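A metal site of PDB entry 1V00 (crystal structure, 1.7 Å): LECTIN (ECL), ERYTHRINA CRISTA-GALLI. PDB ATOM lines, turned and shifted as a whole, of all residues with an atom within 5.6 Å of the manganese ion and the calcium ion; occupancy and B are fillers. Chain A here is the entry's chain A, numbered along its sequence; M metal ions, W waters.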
ATOM      1  N   ASP A  89       0.662 -10.450  -3.976  1.00  0.00           N
ATOM      2  CA  ASP A  89      -0.619 -10.759  -3.345  1.00  0.00           C
ATOM      3  C   ASP A  89      -1.089 -12.176  -3.687  1.00  0.00           C
ATOM      4  O   ASP A  89      -1.901 -12.758  -2.971  1.00  0.00           O
ATOM      5  CB  ASP A  89      -1.699  -9.753  -3.808  1.00  0.00           C
ATOM      6  CG  ASP A  89      -1.863  -8.582  -2.857  1.00  0.00           C
ATOM      7  OD1 ASP A  89      -1.356  -7.483  -3.167  1.00  0.00           O
ATOM      8  OD2 ASP A  89      -2.494  -8.778  -1.799  1.00  0.00           O
ATOM      9  N   GLY A 107      -4.999  -7.290  -3.407  1.00  0.00           N
ATOM     10  CA  GLY A 107      -5.748  -8.432  -2.894  1.00  0.00           C
ATOM     11  C   GLY A 107      -6.875  -8.950  -3.765  1.00  0.00           C
ATOM     12  O   GLY A 107      -7.350 -10.070  -3.552  1.00  0.00           O
ATOM     13  N   GLU A 127      -7.842 -19.548  -6.190  1.00  0.00           N
ATOM     14  CA  GLU A 127      -6.718 -18.682  -5.850  1.00  0.00           C
ATOM     15  C   GLU A 127      -5.610 -19.343  -5.063  1.00  0.00           C
ATOM     16  O   GLU A 127      -5.822 -20.342  -4.371  1.00  0.00           O
ATOM     17  CB  GLU A 127      -7.224 -17.480  -5.052  1.00  0.00           C
ATOM     18  CG  GLU A 127      -7.900 -17.875  -3.746  1.00  0.00           C
ATOM     19  CD  GLU A 127      -8.204 -16.700  -2.840  1.00  0.00           C
ATOM     20  OE1 GLU A 127      -8.865 -15.736  -3.302  1.00  0.00           O
ATOM     21  OE2 GLU A 127      -7.783 -16.723  -1.665  1.00  0.00           O
ATOM     22  N   ASP A 129      -3.374 -17.598  -2.755  1.00  0.00           N
ATOM     23  CA  ASP A 129      -3.260 -16.349  -2.028  1.00  0.00           C
ATOM     24  C   ASP A 129      -2.102 -16.247  -1.049  1.00  0.00           C
ATOM     25  O   ASP A 129      -1.994 -17.043  -0.119  1.00  0.00           O
ATOM     26  CB  ASP A 129      -4.590 -16.158  -1.312  1.00  0.00           C
ATOM     27  CG  ASP A 129      -4.815 -14.767  -0.868  1.00  0.00           C
ATOM     28  OD1 ASP A 129      -5.972 -14.461  -0.493  1.00  0.00           O
ATOM     29  OD2 ASP A 129      -3.847 -13.974  -0.883  1.00  0.00           O
ATOM     30  N   THR A 130      -1.250 -15.241  -1.233  1.00  0.00           N
ATOM     31  CA  THR A 130      -0.077 -15.085  -0.392  1.00  0.00           C
ATOM     32  C   THR A 130      -0.096 -13.995   0.667  1.00  0.00           C
ATOM     33  O   THR A 130       0.824 -13.903   1.487  1.00  0.00           O
ATOM     34  CB  THR A 130       1.160 -14.850  -1.269  1.00  0.00           C
ATOM     35  OG1 THR A 130       0.922 -13.689  -2.089  1.00  0.00           O
ATOM     36  CG2 THR A 130       1.429 -16.061  -2.154  1.00  0.00           C
ATOM     37  N   PHE A 131      -1.131 -13.149   0.668  1.00  0.00           N
ATOM     38  CA  PHE A 131      -1.210 -12.069   1.641  1.00  0.00           C
ATOM     39  C   PHE A 131      -2.558 -12.112   2.346  1.00  0.00           C
ATOM     40  O   PHE A 131      -3.579 -12.180   1.700  1.00  0.00           O
ATOM     41  CB  PHE A 131      -1.050 -10.704   0.940  1.00  0.00           C
ATOM     42  CG  PHE A 131      -1.129  -9.536   1.882  1.00  0.00           C
ATOM     43  CD1 PHE A 131       0.019  -9.046   2.505  1.00  0.00           C
ATOM     44  CD2 PHE A 131      -2.354  -8.965   2.189  1.00  0.00           C
ATOM     45  CE1 PHE A 131      -0.052  -7.990   3.425  1.00  0.00           C
ATOM     46  CE2 PHE A 131      -2.447  -7.915   3.111  1.00  0.00           C
ATOM     47  CZ  PHE A 131      -1.285  -7.426   3.733  1.00  0.00           C
ATOM     48  N   SER A 132      -2.567 -12.065   3.675  1.00  0.00           N
ATOM     49  CA  SER A 132      -3.828 -12.112   4.391  1.00  0.00           C
ATOM     50  C   SER A 132      -4.523 -10.746   4.518  1.00  0.00           C
ATOM     51  O   SER A 132      -4.118  -9.902   5.316  1.00  0.00           O
ATOM     52  CB  SER A 132      -3.618 -12.701   5.796  1.00  0.00           C
ATOM     53  OG  SER A 132      -4.856 -12.805   6.483  1.00  0.00           O
ATOM     54  N   ASN A 133      -5.552 -10.542   3.698  1.00  0.00           N
ATOM     55  CA  ASN A 133      -6.327  -9.298   3.731  1.00  0.00           C
ATOM     56  C   ASN A 133      -7.401  -9.396   4.805  1.00  0.00           C
ATOM     57  O   ASN A 133      -7.598 -10.457   5.389  1.00  0.00           O
ATOM     58  CB  ASN A 133      -6.992  -9.026   2.373  1.00  0.00           C
ATOM     59  CG  ASN A 133      -5.984  -8.738   1.274  1.00  0.00           C
ATOM     60  OD1 ASN A 133      -5.508  -9.653   0.618  1.00  0.00           O
ATOM     61  ND2 ASN A 133      -5.658  -7.470   1.081  1.00  0.00           N
ATOM     62  N   TRP A 135     -10.489  -9.776   4.631  1.00  0.00           N
ATOM     63  CA  TRP A 135     -11.509 -10.770   4.308  1.00  0.00           C
ATOM     64  C   TRP A 135     -10.947 -12.198   4.229  1.00  0.00           C
ATOM     65  O   TRP A 135     -11.681 -13.148   3.972  1.00  0.00           O
ATOM     66  CB  TRP A 135     -12.149 -10.422   2.966  1.00  0.00           C
ATOM     67  CG  TRP A 135     -11.138 -10.345   1.845  1.00  0.00           C
ATOM     68  CD1 TRP A 135     -10.559 -11.401   1.195  1.00  0.00           C
ATOM     69  CD2 TRP A 135     -10.532  -9.166   1.311  1.00  0.00           C
ATOM     70  NE1 TRP A 135      -9.632 -10.949   0.282  1.00  0.00           N
ATOM     71  CE2 TRP A 135      -9.602  -9.576   0.333  1.00  0.00           C
ATOM     72  CE3 TRP A 135     -10.686  -7.796   1.563  1.00  0.00           C
ATOM     73  CZ2 TRP A 135      -8.820  -8.665  -0.388  1.00  0.00           C
ATOM     74  CZ3 TRP A 135      -9.919  -6.884   0.844  1.00  0.00           C
ATOM     75  CH2 TRP A 135      -8.996  -7.330  -0.127  1.00  0.00           C
ATOM     76  N   ASP A 136      -9.649 -12.320   4.484  1.00  0.00           N
ATOM     77  CA  ASP A 136      -8.967 -13.612   4.405  1.00  0.00           C
ATOM     78  C   ASP A 136      -8.757 -14.335   5.727  1.00  0.00           C
ATOM     79  O   ASP A 136      -8.822 -13.743   6.802  1.00  0.00           O
ATOM     80  CB  ASP A 136      -7.547 -13.453   3.866  1.00  0.00           C
ATOM     81  CG  ASP A 136      -7.496 -13.268   2.383  1.00  0.00           C
ATOM     82  OD1 ASP A 136      -8.166 -14.029   1.672  1.00  0.00           O
ATOM     83  OD2 ASP A 136      -6.755 -12.368   1.949  1.00  0.00           O
ATOM     84  N   PRO A 137      -8.490 -15.649   5.640  1.00  0.00           N
ATOM     85  CA  PRO A 137      -8.239 -16.434   6.839  1.00  0.00           C
ATOM     86  C   PRO A 137      -6.831 -15.936   7.163  1.00  0.00           C
ATOM     87  O   PRO A 137      -6.139 -15.404   6.283  1.00  0.00           O
ATOM     88  CB  PRO A 137      -8.252 -17.877   6.315  1.00  0.00           C
ATOM     89  CG  PRO A 137      -7.820 -17.737   4.888  1.00  0.00           C
ATOM     90  CD  PRO A 137      -8.597 -16.514   4.455  1.00  0.00           C
ATOM     91  N   HIS A 142      -2.578 -19.655   1.051  1.00  0.00           N
ATOM     92  CA  HIS A 142      -3.703 -20.573   1.120  1.00  0.00           C
ATOM     93  C   HIS A 142      -4.355 -20.700  -0.237  1.00  0.00           C
ATOM     94  O   HIS A 142      -4.296 -19.772  -1.062  1.00  0.00           O
ATOM     95  CB  HIS A 142      -4.760 -20.114   2.157  1.00  0.00           C
ATOM     96  CG  HIS A 142      -5.325 -18.747   1.907  1.00  0.00           C
ATOM     97  ND1 HIS A 142      -4.889 -17.628   2.567  1.00  0.00           N
ATOM     98  CD2 HIS A 142      -6.305 -18.330   1.072  1.00  0.00           C
ATOM     99  CE1 HIS A 142      -5.577 -16.576   2.157  1.00  0.00           C
ATOM    100  NE2 HIS A 142      -6.441 -16.981   1.239  1.00  0.00           N
ATOM    101  N   ILE A 150     -14.021 -12.493  -3.738  1.00  0.00           N
ATOM    102  CA  ILE A 150     -12.628 -12.717  -3.363  1.00  0.00           C
ATOM    103  C   ILE A 150     -12.635 -13.365  -1.971  1.00  0.00           C
ATOM    104  O   ILE A 150     -11.616 -13.905  -1.516  1.00  0.00           O
ATOM    105  CB  ILE A 150     -11.834 -11.393  -3.337  1.00  0.00           C
ATOM    106  CG1 ILE A 150     -10.335 -11.662  -3.139  1.00  0.00           C
ATOM    107  CG2 ILE A 150     -12.337 -10.500  -2.205  1.00  0.00           C
ATOM    108  CD1 ILE A 150      -9.650 -12.354  -4.310  1.00  0.00           C
ATOM    109  N   SER A 152     -13.292 -16.244  -0.335  1.00  0.00           N
ATOM    110  CA  SER A 152     -13.529 -17.634  -0.709  1.00  0.00           C
ATOM    111  C   SER A 152     -14.483 -18.398   0.206  1.00  0.00           C
ATOM    112  O   SER A 152     -14.561 -18.174   1.429  1.00  0.00           O
ATOM    113  CB  SER A 152     -12.180 -18.367  -0.874  1.00  0.00           C
ATOM    114  OG  SER A 152     -11.383 -17.745  -1.867  1.00  0.00           O
ATOM    115  N   THR A 155     -11.169 -22.435   2.044  1.00  0.00           N
ATOM    116  CA  THR A 155      -9.727 -22.189   1.925  1.00  0.00           C
ATOM    117  C   THR A 155      -8.941 -23.330   2.548  1.00  0.00           C
ATOM    118  O   THR A 155      -9.454 -24.073   3.388  1.00  0.00           O
ATOM    119  CB  THR A 155      -9.303 -20.864   2.596  1.00  0.00           C
ATOM    120  OG1 THR A 155      -9.708 -20.873   3.972  1.00  0.00           O
ATOM    121  CG2 THR A 155      -9.948 -19.686   1.891  1.00  0.00           C
HETATM  122 MN    MN M   1      -7.749 -15.444   0.074  1.00  0.00          MN
HETATM  123 CA    CA M   2      -5.299 -12.080   0.003  1.00  0.00          CA
HETATM  124  O   HOH W   1      -3.597 -11.094  -1.627  1.00  0.00           O
HETATM  125  O   HOH W   2      -7.269 -11.810  -1.559  1.00  0.00           O
HETATM  126  O   HOH W   3      -8.927 -14.081  -1.344  1.00  0.00           O
HETATM  127  O   HOH W   4      -9.627 -16.343   0.792  1.00  0.00           O
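Water W3 lies within hydrogen-bond range of OE1 of Glu 127 (2.6 Å) and O of Ile 150 (2.7 Å).
Water W2 lies within hydrogen-bond range of the backbone carbonyl oxygen of Gly 107 (2.6 Å) and the indole nitrogen of Trp 135 (3.1 Å).
The calcium ion is bound by O of Phe 131, OD2 of Asp 136, OD1 of Asn 133, OD1 of Asp 129, water W2, OD2 of Asp 129 and water W1.
The calcium ion has seven donor atoms within binding distance.
The manganese ion is bound by the side-chain carboxylate (OD1) of Asp 129, the side-chain carboxylate (OE2) of Glu 127, the side-chain carboxylate (OD1) of Asp 136, water W4, water W3 and a ring nitrogen (NE2) of His 142.
The manganese ion has six donor atoms within binding distance.
Four residues have an atom within 4 Å of the manganese ion: Glu 127, Asp 129, Asp 136 and His 142.
Along chain A the residues within 4 Å of the manganese ion span positions 127 to 142.
The nearest printed residue that does not touch the manganese ion is Ile 150 (4.5 Å).
Four residues have an atom within 4 Å of the calcium ion: Asp 129, Phe 131, Asn 133 and Asp 136.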
